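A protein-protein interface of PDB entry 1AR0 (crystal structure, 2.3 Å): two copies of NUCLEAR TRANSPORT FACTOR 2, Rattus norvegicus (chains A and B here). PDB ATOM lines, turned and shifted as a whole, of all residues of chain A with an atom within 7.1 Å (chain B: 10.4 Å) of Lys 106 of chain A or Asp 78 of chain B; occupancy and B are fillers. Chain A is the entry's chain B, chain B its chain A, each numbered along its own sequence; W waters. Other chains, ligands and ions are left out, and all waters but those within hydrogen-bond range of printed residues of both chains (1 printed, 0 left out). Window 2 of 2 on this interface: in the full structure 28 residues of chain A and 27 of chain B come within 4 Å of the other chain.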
ATOM      1  N   ILE A  34       5.791  -1.862   7.729  1.00  0.00           N
ATOM      2  CA  ILE A  34       6.773  -0.920   7.176  1.00  0.00           C
ATOM      3  C   ILE A  34       6.833  -1.254   5.703  1.00  0.00           C
ATOM      4  O   ILE A  34       6.342  -2.323   5.298  1.00  0.00           O
ATOM      5  CB  ILE A  34       8.139  -1.009   7.846  1.00  0.00           C
ATOM      6  CG1 ILE A  34       8.579  -2.454   8.017  1.00  0.00           C
ATOM      7  CG2 ILE A  34       8.126  -0.333   9.209  1.00  0.00           C
ATOM      8  CD1 ILE A  34      10.063  -2.611   8.244  1.00  0.00           C
ATOM      9  N   THR A  76      12.999 -11.504  21.691  1.00  0.00           N
ATOM     10  CA  THR A  76      14.119 -12.180  21.020  1.00  0.00           C
ATOM     11  C   THR A  76      15.375 -11.507  21.549  1.00  0.00           C
ATOM     12  O   THR A  76      15.387 -10.365  22.013  1.00  0.00           O
ATOM     13  CB  THR A  76      14.098 -11.997  19.498  1.00  0.00           C
ATOM     14  OG1 THR A  76      14.436 -10.614  19.213  1.00  0.00           O
ATOM     15  CG2 THR A  76      12.718 -12.281  18.911  1.00  0.00           C
ATOM     16  N   ASP A  78      17.751  -9.920  19.767  1.00  0.00           N
ATOM     17  CA  ASP A  78      17.999  -8.700  19.058  1.00  0.00           C
ATOM     18  C   ASP A  78      16.915  -7.668  19.150  1.00  0.00           C
ATOM     19  O   ASP A  78      16.638  -6.856  18.267  1.00  0.00           O
ATOM     20  CB  ASP A  78      18.254  -8.967  17.566  1.00  0.00           C
ATOM     21  CG  ASP A  78      18.967 -10.246  17.229  1.00  0.00           C
ATOM     22  OD1 ASP A  78      20.003 -10.532  17.860  1.00  0.00           O
ATOM     23  OD2 ASP A  78      18.495 -11.005  16.350  1.00  0.00           O
ATOM     24  N   SER A  79      16.198  -7.580  20.269  1.00  0.00           N
ATOM     25  CA  SER A  79      15.188  -6.617  20.603  1.00  0.00           C
ATOM     26  C   SER A  79      13.888  -6.715  19.847  1.00  0.00           C
ATOM     27  O   SER A  79      13.222  -5.708  19.624  1.00  0.00           O
ATOM     28  CB  SER A  79      15.823  -5.217  20.455  1.00  0.00           C
ATOM     29  OG  SER A  79      16.958  -5.062  21.292  1.00  0.00           O
ATOM     30  N   CYS A  80      13.462  -7.866  19.369  1.00  0.00           N
ATOM     31  CA  CYS A  80      12.188  -7.955  18.650  1.00  0.00           C
ATOM     32  C   CYS A  80      11.209  -8.650  19.574  1.00  0.00           C
ATOM     33  O   CYS A  80      11.574  -9.054  20.682  1.00  0.00           O
ATOM     34  CB  CYS A  80      12.363  -8.693  17.336  1.00  0.00           C
ATOM     35  SG  CYS A  80      13.430  -7.804  16.164  1.00  0.00           S
ATOM     36  N   ILE A  81       9.937  -8.714  19.223  1.00  0.00           N
ATOM     37  CA  ILE A  81       8.904  -9.458  19.926  1.00  0.00           C
ATOM     38  C   ILE A  81       8.255 -10.387  18.897  1.00  0.00           C
ATOM     39  O   ILE A  81       7.976 -10.052  17.752  1.00  0.00           O
ATOM     40  CB  ILE A  81       7.901  -8.547  20.630  1.00  0.00           C
ATOM     41  CG1 ILE A  81       8.443  -7.906  21.929  1.00  0.00           C
ATOM     42  CG2 ILE A  81       6.619  -9.288  21.054  1.00  0.00           C
ATOM     43  CD1 ILE A  81       7.927  -6.539  22.183  1.00  0.00           C
ATOM     44  N   LEU A 104       6.078 -10.843  13.768  1.00  0.00           N
ATOM     45  CA  LEU A 104       7.407 -10.488  14.282  1.00  0.00           C
ATOM     46  C   LEU A 104       7.400  -8.970  14.382  1.00  0.00           C
ATOM     47  O   LEU A 104       7.087  -8.337  13.387  1.00  0.00           O
ATOM     48  CB  LEU A 104       8.594 -10.957  13.475  1.00  0.00           C
ATOM     49  CG  LEU A 104       9.976 -10.621  14.071  1.00  0.00           C
ATOM     50  CD1 LEU A 104      10.224 -11.309  15.388  1.00  0.00           C
ATOM     51  CD2 LEU A 104      11.087 -11.059  13.116  1.00  0.00           C
ATOM     52  N   LEU A 105       7.580  -8.419  15.571  1.00  0.00           N
ATOM     53  CA  LEU A 105       7.493  -7.002  15.800  1.00  0.00           C
ATOM     54  C   LEU A 105       8.867  -6.377  16.046  1.00  0.00           C
ATOM     55  O   LEU A 105       9.685  -7.038  16.667  1.00  0.00           O
ATOM     56  CB  LEU A 105       6.608  -6.732  17.015  1.00  0.00           C
ATOM     57  CG  LEU A 105       5.206  -7.345  17.077  1.00  0.00           C
ATOM     58  CD1 LEU A 105       4.515  -6.812  18.331  1.00  0.00           C
ATOM     59  CD2 LEU A 105       4.373  -7.055  15.843  1.00  0.00           C
ATOM     60  N   LYS A 106       9.090  -5.150  15.597  1.00  0.00           N
ATOM     61  CA  LYS A 106      10.410  -4.534  15.761  1.00  0.00           C
ATOM     62  C   LYS A 106      10.233  -3.057  16.060  1.00  0.00           C
ATOM     63  O   LYS A 106       9.242  -2.485  15.618  1.00  0.00           O
ATOM     64  CB  LYS A 106      11.255  -4.655  14.503  1.00  0.00           C
ATOM     65  CG  LYS A 106      12.663  -4.094  14.601  1.00  0.00           C
ATOM     66  CD  LYS A 106      13.466  -4.428  13.344  1.00  0.00           C
ATOM     67  CE  LYS A 106      14.882  -3.866  13.479  1.00  0.00           C
ATOM     68  NZ  LYS A 106      15.644  -4.680  14.465  1.00  0.00           N
ATOM     69  N   ASN A 107      11.015  -2.562  17.002  1.00  0.00           N
ATOM     70  CA  ASN A 107      10.910  -1.145  17.339  1.00  0.00           C
ATOM     71  C   ASN A 107      11.698  -0.313  16.340  1.00  0.00           C
ATOM     72  O   ASN A 107      12.915  -0.384  16.254  1.00  0.00           O
ATOM     73  CB  ASN A 107      11.387  -0.916  18.767  1.00  0.00           C
ATOM     74  CG  ASN A 107      11.014   0.457  19.252  1.00  0.00           C
ATOM     75  OD1 ASN A 107      11.533   1.472  18.810  1.00  0.00           O
ATOM     76  ND2 ASN A 107      10.066   0.553  20.172  1.00  0.00           N
ATOM     77  N   ILE A 108      11.025   0.388  15.459  1.00  0.00           N
ATOM     78  CA  ILE A 108      11.604   1.199  14.405  1.00  0.00           C
ATOM     79  C   ILE A 108      11.015   2.581  14.594  1.00  0.00           C
ATOM     80  O   ILE A 108       9.819   2.839  14.543  1.00  0.00           O
ATOM     81  CB  ILE A 108      11.365   0.715  12.977  1.00  0.00           C
ATOM     82  CG1 ILE A 108      12.194  -0.518  12.609  1.00  0.00           C
ATOM     83  CG2 ILE A 108      11.703   1.751  11.905  1.00  0.00           C
ATOM     84  CD1 ILE A 108      11.386  -1.651  12.039  1.00  0.00           C
ATOM     85  N   ASN A 109      11.893   3.563  14.812  1.00  0.00           N
ATOM     86  CA  ASN A 109      11.603   4.968  14.975  1.00  0.00           C
ATOM     87  C   ASN A 109      10.822   5.303  16.226  1.00  0.00           C
ATOM     88  O   ASN A 109       9.887   6.109  16.261  1.00  0.00           O
ATOM     89  CB  ASN A 109      10.863   5.521  13.758  1.00  0.00           C
ATOM     90  CG  ASN A 109      11.583   5.543  12.437  1.00  0.00           C
ATOM     91  OD1 ASN A 109      10.952   5.573  11.386  1.00  0.00           O
ATOM     92  ND2 ASN A 109      12.901   5.452  12.439  1.00  0.00           N
ATOM     93  N   ALA A 111       8.515   3.255  17.672  1.00  0.00           N
ATOM     94  CA  ALA A 111       7.230   2.605  17.604  1.00  0.00           C
ATOM     95  C   ALA A 111       7.367   1.154  17.201  1.00  0.00           C
ATOM     96  O   ALA A 111       8.232   0.811  16.402  1.00  0.00           O
ATOM     97  CB  ALA A 111       6.371   3.321  16.568  1.00  0.00           C
ATOM     98  N   TRP A 112       6.465   0.321  17.707  1.00  0.00           N
ATOM     99  CA  TRP A 112       6.519  -1.093  17.354  1.00  0.00           C
ATOM    100  C   TRP A 112       5.785  -1.314  16.063  1.00  0.00           C
ATOM    101  O   TRP A 112       4.666  -0.834  15.891  1.00  0.00           O
ATOM    102  CB  TRP A 112       5.964  -1.918  18.510  1.00  0.00           C
ATOM    103  CG  TRP A 112       6.952  -1.909  19.644  1.00  0.00           C
ATOM    104  CD1 TRP A 112       7.011  -1.013  20.671  1.00  0.00           C
ATOM    105  CD2 TRP A 112       8.029  -2.809  19.833  1.00  0.00           C
ATOM    106  NE1 TRP A 112       8.043  -1.335  21.494  1.00  0.00           N
ATOM    107  CE2 TRP A 112       8.694  -2.425  21.009  1.00  0.00           C
ATOM    108  CE3 TRP A 112       8.488  -3.924  19.163  1.00  0.00           C
ATOM    109  CZ2 TRP A 112       9.803  -3.101  21.505  1.00  0.00           C
ATOM    110  CZ3 TRP A 112       9.611  -4.591  19.604  1.00  0.00           C
ATOM    111  CH2 TRP A 112      10.228  -4.181  20.790  1.00  0.00           C
ATOM    112  N   VAL A 113       6.394  -1.937  15.075  1.00  0.00           N
ATOM    113  CA  VAL A 113       5.741  -2.218  13.799  1.00  0.00           C
ATOM    114  C   VAL A 113       5.872  -3.697  13.516  1.00  0.00           C
ATOM    115  O   VAL A 113       6.753  -4.334  14.087  1.00  0.00           O
ATOM    116  CB  VAL A 113       6.338  -1.479  12.602  1.00  0.00           C
ATOM    117  CG1 VAL A 113       5.973  -0.001  12.563  1.00  0.00           C
ATOM    118  CG2 VAL A 113       7.856  -1.627  12.584  1.00  0.00           C
ATOM    119  N   CYS A 114       5.083  -4.232  12.589  1.00  0.00           N
ATOM    120  CA  CYS A 114       5.162  -5.630  12.233  1.00  0.00           C
ATOM    121  C   CYS A 114       6.067  -5.830  11.031  1.00  0.00           C
ATOM    122  O   CYS A 114       5.785  -5.247   9.982  1.00  0.00           O
ATOM    123  CB  CYS A 114       3.749  -6.147  11.858  1.00  0.00           C
ATOM    124  SG  CYS A 114       3.870  -7.905  11.422  1.00  0.00           S
ATOM    125  N   THR A 115       7.081  -6.689  11.094  1.00  0.00           N
ATOM    126  CA  THR A 115       7.920  -6.787   9.896  1.00  0.00           C
ATOM    127  C   THR A 115       7.507  -7.995   9.115  1.00  0.00           C
ATOM    128  O   THR A 115       7.838  -8.173   7.940  1.00  0.00           O
ATOM    129  CB  THR A 115       9.427  -6.803  10.197  1.00  0.00           C
ATOM    130  OG1 THR A 115       9.758  -7.857  11.103  1.00  0.00           O
ATOM    131  CG2 THR A 115       9.926  -5.505  10.800  1.00  0.00           C
ATOM    132  N   GLN B  74      10.277 -17.257   6.369  1.00  0.00           N
ATOM    133  CA  GLN B  74      10.596 -15.931   5.899  1.00  0.00           C
ATOM    134  C   GLN B  74      11.932 -15.459   6.468  1.00  0.00           C
ATOM    135  O   GLN B  74      12.318 -15.781   7.568  1.00  0.00           O
ATOM    136  CB  GLN B  74       9.585 -14.856   6.300  1.00  0.00           C
ATOM    137  CG  GLN B  74       8.196 -14.893   5.691  1.00  0.00           C
ATOM    138  CD  GLN B  74       7.205 -13.972   6.314  1.00  0.00           C
ATOM    139  OE1 GLN B  74       7.507 -13.302   7.304  1.00  0.00           O
ATOM    140  NE2 GLN B  74       6.048 -13.946   5.683  1.00  0.00           N
ATOM    141  N   PRO B  75      12.631 -14.578   5.726  1.00  0.00           N
ATOM    142  CA  PRO B  75      13.828 -13.931   6.242  1.00  0.00           C
ATOM    143  C   PRO B  75      13.400 -12.773   7.142  1.00  0.00           C
ATOM    144  O   PRO B  75      12.339 -12.193   6.911  1.00  0.00           O
ATOM    145  CB  PRO B  75      14.514 -13.368   5.004  1.00  0.00           C
ATOM    146  CG  PRO B  75      13.375 -13.045   4.056  1.00  0.00           C
ATOM    147  CD  PRO B  75      12.320 -14.111   4.349  1.00  0.00           C
ATOM    148  N   THR B  76      14.122 -12.444   8.195  1.00  0.00           N
ATOM    149  CA  THR B  76      13.751 -11.280   9.000  1.00  0.00           C
ATOM    150  C   THR B  76      14.754 -10.206   8.600  1.00  0.00           C
ATOM    151  O   THR B  76      15.825 -10.468   8.078  1.00  0.00           O
ATOM    152  CB  THR B  76      13.861 -11.573  10.492  1.00  0.00           C
ATOM    153  OG1 THR B  76      15.245 -11.650  10.842  1.00  0.00           O
ATOM    154  CG2 THR B  76      13.213 -12.909  10.900  1.00  0.00           C
ATOM    155  N   PRO B  77      14.530  -8.947   8.975  1.00  0.00           N
ATOM    156  CA  PRO B  77      15.397  -7.818   8.716  1.00  0.00           C
ATOM    157  C   PRO B  77      16.773  -7.841   9.340  1.00  0.00           C
ATOM    158  O   PRO B  77      17.737  -7.384   8.709  1.00  0.00           O
ATOM    159  CB  PRO B  77      14.691  -6.571   9.211  1.00  0.00           C
ATOM    160  CG  PRO B  77      13.246  -6.952   9.366  1.00  0.00           C
ATOM    161  CD  PRO B  77      13.290  -8.454   9.642  1.00  0.00           C
ATOM    162  N   ASP B  78      17.024  -8.511  10.450  1.00  0.00           N
ATOM    163  CA  ASP B  78      18.320  -8.669  11.052  1.00  0.00           C
ATOM    164  C   ASP B  78      19.008  -9.957  10.652  1.00  0.00           C
ATOM    165  O   ASP B  78      19.809 -10.513  11.407  1.00  0.00           O
ATOM    166  CB  ASP B  78      18.202  -8.666  12.576  1.00  0.00           C
ATOM    167  CG  ASP B  78      17.391  -7.564  13.186  1.00  0.00           C
ATOM    168  OD1 ASP B  78      18.012  -6.523  13.487  1.00  0.00           O
ATOM    169  OD2 ASP B  78      16.168  -7.721  13.393  1.00  0.00           O
ATOM    170  N   SER B  79      18.691 -10.606   9.559  1.00  0.00           N
ATOM    171  CA  SER B  79      19.277 -11.787   9.015  1.00  0.00           C
ATOM    172  C   SER B  79      18.880 -13.092   9.640  1.00  0.00           C
ATOM    173  O   SER B  79      19.580 -14.075   9.436  1.00  0.00           O
ATOM    174  CB  SER B  79      20.829 -11.628   9.043  1.00  0.00           C
ATOM    175  OG  SER B  79      21.134 -10.895   7.859  1.00  0.00           O
ATOM    176  N   CYS B  80      17.755 -13.140  10.352  1.00  0.00           N
ATOM    177  CA  CYS B  80      17.316 -14.376  10.973  1.00  0.00           C
ATOM    178  C   CYS B  80      16.322 -15.035  10.037  1.00  0.00           C
ATOM    179  O   CYS B  80      15.899 -14.517   9.004  1.00  0.00           O
ATOM    180  CB  CYS B  80      16.729 -14.021  12.342  1.00  0.00           C
ATOM    181  SG  CYS B  80      17.991 -13.488  13.554  1.00  0.00           S
ATOM    182  N   ILE B  81      15.987 -16.278  10.319  1.00  0.00           N
ATOM    183  CA  ILE B  81      14.983 -17.028   9.588  1.00  0.00           C
ATOM    184  C   ILE B  81      13.824 -17.276  10.571  1.00  0.00           C
ATOM    185  O   ILE B  81      13.996 -17.833  11.649  1.00  0.00           O
ATOM    186  CB  ILE B  81      15.504 -18.310   8.960  1.00  0.00           C
ATOM    187  CG1 ILE B  81      16.553 -18.045   7.847  1.00  0.00           C
ATOM    188  CG2 ILE B  81      14.368 -19.146   8.359  1.00  0.00           C
ATOM    189  CD1 ILE B  81      17.348 -19.263   7.460  1.00  0.00           C
ATOM    190  N   ILE B  82      12.619 -16.893  10.206  1.00  0.00           N
ATOM    191  CA  ILE B  82      11.450 -17.168  11.038  1.00  0.00           C
ATOM    192  C   ILE B  82      10.550 -18.164  10.336  1.00  0.00           C
ATOM    193  O   ILE B  82      10.240 -18.022   9.158  1.00  0.00           O
ATOM    194  CB  ILE B  82      10.763 -15.880  11.476  1.00  0.00           C
ATOM    195  CG1 ILE B  82       9.820 -16.156  12.648  1.00  0.00           C
ATOM    196  CG2 ILE B  82      10.044 -15.159  10.372  1.00  0.00           C
ATOM    197  CD1 ILE B  82       9.308 -14.911  13.335  1.00  0.00           C
ATOM    198  N   LEU B 104      12.512 -19.313  15.541  1.00  0.00           N
ATOM    199  CA  LEU B 104      13.283 -18.152  15.077  1.00  0.00           C
ATOM    200  C   LEU B 104      14.745 -18.604  15.057  1.00  0.00           C
ATOM    201  O   LEU B 104      15.239 -18.989  16.111  1.00  0.00           O
ATOM    202  CB  LEU B 104      13.138 -16.896  15.912  1.00  0.00           C
ATOM    203  CG  LEU B 104      13.976 -15.697  15.427  1.00  0.00           C
ATOM    204  CD1 LEU B 104      13.378 -15.083  14.161  1.00  0.00           C
ATOM    205  CD2 LEU B 104      14.096 -14.590  16.457  1.00  0.00           C
ATOM    206  N   LEU B 105      15.354 -18.691  13.893  1.00  0.00           N
ATOM    207  CA  LEU B 105      16.711 -19.154  13.710  1.00  0.00           C
ATOM    208  C   LEU B 105      17.730 -18.043  13.468  1.00  0.00           C
ATOM    209  O   LEU B 105      17.464 -17.069  12.762  1.00  0.00           O
ATOM    210  CB  LEU B 105      16.828 -20.132  12.541  1.00  0.00           C
ATOM    211  CG  LEU B 105      15.770 -21.243  12.475  1.00  0.00           C
ATOM    212  CD1 LEU B 105      15.998 -22.051  11.216  1.00  0.00           C
ATOM    213  CD2 LEU B 105      15.816 -22.120  13.704  1.00  0.00           C
ATOM    214  N   LYS B 106      18.923 -18.268  14.012  1.00  0.00           N
ATOM    215  CA  LYS B 106      20.006 -17.294  13.897  1.00  0.00           C
ATOM    216  C   LYS B 106      21.343 -17.986  13.671  1.00  0.00           C
ATOM    217  O   LYS B 106      21.547 -19.108  14.129  1.00  0.00           O
ATOM    218  CB  LYS B 106      20.074 -16.440  15.153  1.00  0.00           C
ATOM    219  CG  LYS B 106      20.940 -15.196  15.005  1.00  0.00           C
ATOM    220  CD  LYS B 106      21.243 -14.637  16.380  1.00  0.00           C
ATOM    221  CE  LYS B 106      22.413 -13.661  16.318  1.00  0.00           C
ATOM    222  NZ  LYS B 106      21.884 -12.259  16.248  1.00  0.00           N
ATOM    223  N   ASN B 107      22.125 -17.432  12.745  1.00  0.00           N
ATOM    224  CA  ASN B 107      23.398 -18.066  12.381  1.00  0.00           C
ATOM    225  C   ASN B 107      24.504 -17.585  13.305  1.00  0.00           C
ATOM    226  O   ASN B 107      24.840 -16.421  13.405  1.00  0.00           O
ATOM    227  CB  ASN B 107      23.778 -17.822  10.931  1.00  0.00           C
ATOM    228  CG  ASN B 107      24.886 -18.721  10.455  1.00  0.00           C
ATOM    229  OD1 ASN B 107      24.706 -19.616   9.639  1.00  0.00           O
ATOM    230  ND2 ASN B 107      26.113 -18.570  10.922  1.00  0.00           N
ATOM    231  N   ILE B 108      24.966 -18.493  14.151  1.00  0.00           N
ATOM    232  CA  ILE B 108      26.007 -18.231  15.143  1.00  0.00           C
ATOM    233  C   ILE B 108      27.102 -19.274  14.952  1.00  0.00           C
ATOM    234  O   ILE B 108      26.861 -20.472  14.990  1.00  0.00           O
ATOM    235  CB  ILE B 108      25.502 -18.240  16.588  1.00  0.00           C
ATOM    236  CG1 ILE B 108      24.617 -17.055  16.968  1.00  0.00           C
ATOM    237  CG2 ILE B 108      26.651 -18.218  17.605  1.00  0.00           C
ATOM    238  CD1 ILE B 108      23.460 -17.329  17.887  1.00  0.00           C
ATOM    239  N   TRP B 112      23.216 -22.539  12.117  1.00  0.00           N
ATOM    240  CA  TRP B 112      21.887 -22.003  12.387  1.00  0.00           C
ATOM    241  C   TRP B 112      21.386 -22.604  13.689  1.00  0.00           C
ATOM    242  O   TRP B 112      21.316 -23.816  13.842  1.00  0.00           O
ATOM    243  CB  TRP B 112      20.956 -22.353  11.209  1.00  0.00           C
ATOM    244  CG  TRP B 112      21.370 -21.516  10.037  1.00  0.00           C
ATOM    245  CD1 TRP B 112      22.192 -21.897   9.023  1.00  0.00           C
ATOM    246  CD2 TRP B 112      21.007 -20.164   9.777  1.00  0.00           C
ATOM    247  NE1 TRP B 112      22.345 -20.860   8.148  1.00  0.00           N
ATOM    248  CE2 TRP B 112      21.640 -19.781   8.587  1.00  0.00           C
ATOM    249  CE3 TRP B 112      20.176 -19.252  10.397  1.00  0.00           C
ATOM    250  CZ2 TRP B 112      21.489 -18.524   8.017  1.00  0.00           C
ATOM    251  CZ3 TRP B 112      20.044 -17.986   9.874  1.00  0.00           C
ATOM    252  CH2 TRP B 112      20.688 -17.644   8.680  1.00  0.00           C
ATOM    253  N   THR B 115      16.910 -19.619  18.575  1.00  0.00           N
ATOM    254  CA  THR B 115      16.877 -18.744  19.715  1.00  0.00           C
ATOM    255  C   THR B 115      15.491 -18.737  20.346  1.00  0.00           C
ATOM    256  O   THR B 115      15.294 -18.308  21.494  1.00  0.00           O
ATOM    257  CB  THR B 115      17.288 -17.297  19.418  1.00  0.00           C
ATOM    258  OG1 THR B 115      16.312 -16.616  18.612  1.00  0.00           O
ATOM    259  CG2 THR B 115      18.663 -17.253  18.749  1.00  0.00           C
HETATM  260  O   HOH W   1      17.514 -13.545  17.317  1.00  0.00           O
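Water W1 bridges OD2 of Asp 78 of chain A and SG of Cys 80 of chain B.
OD2 of Asp 78 of chain A lies within hydrogen-bond range of SG of Cys 80 of chain B (3.8 Å). NZ of Lys 106 of chain B lies within salt-bridge range of OD1 of Asp 78 of chain A (3.0 Å). The side-chain amino group (NZ) of Lys 106 of chain A lies within salt-bridge range of the side-chain carboxylate (OD1) of Asp 78 of chain B (3.2 Å).
Thr 76 of chain A touches Leu 104 of chain B (CG2 to CD2, 3.6 Å). Asp 78 of chain B touches Cys 80 of chain A. CD2 of Leu 104 of chain A touches CG2 of Thr 76 of chain B, 3.6 Å away. OG1 of Thr 115 of chain A touches CD of Pro 77 of chain B, at 3.9 Å.
The backbone carbonyl oxygen of Val 113 of chain A is in hydrogen-bond range of the backbone NH of Lys 106 of chain A (2.9 Å). The backbone carbonyl oxygen of Leu 104 of chain B sits at hydrogen-bond distance from the backbone NH of Thr 115 of chain B (3.0 Å). SG of Cys 80 of chain B lies close to O of Leu 105 of chain B, 3.7 Å away. The backbone NH of Cys 80 of chain A sits at hydrogen-bond distance from the side-chain hydroxyl of Thr 76 of chain A. The side-chain hydroxyl of Thr 76 of chain A lies close to the backbone NH of Asp 78 of chain A, 3.4 Å away. The backbone NH of Cys 80 of chain B sits at hydrogen-bond distance from the side-chain hydroxyl of Thr 76 of chain B (3.0 Å).
Printed residues of chain B within 4 Å of Lys 106 of chain A: Asp 78 (3.2 Å). Asp 78 of chain B touches two residues of chain A. No residue of chain B comes within 4 Å of Leu 105 of chain A. No residue of chain B comes within 4 Å of Trp 112 of chain A. No residue of chain B comes within 4 Å of Val 113 of chain A. Printed residues of chain B within 4 Å of Cys 80 of chain A: Asp 78. Printed residues of chain B within 4 Å of Leu 104 of chain A: Thr 76. Of the printed residues of chain A, Thr 76 of chain B touches Leu 104. Of the printed residues of chain B, Asp 78 of chain A touches Cys 80 (3.8 Å) and Lys 106 (3.0 Å). Of the printed residues of chain B, Thr 115 of chain A touches Pro 77. Ser 79 of chain A touches none of the printed residues of chain B. Ile 81 of chain B touches none of the printed residues of chain A.
Among the printed residues, 7 pairs touch across the chains. Among the printed residues, Asp or Glu carboxylates within 4 Å of a Lys or Arg side-chain nitrogen of the other chain: Asp 78 of chain A with Lys 106 of chain B and Lys 106 of chain A with Asp 78 of chain B.
Thr 76 of chain A touches Leu 104 of chain B, and with the chains exchanged Leu 104 of chain A touches Thr 76 of chain B. Asp 78 of chain A touches Cys 80 of chain B, and with the chains exchanged Cys 80 of chain A touches Asp 78 of chain B. Asp 78 of chain A touches Lys 106 of chain B, and with the chains exchanged Lys 106 of chain A touches Asp 78 of chain B. Positions printed for both chains: 76, 78, 79, 80, 81, 104, 105, 106, 107, 108, 112 and 115.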
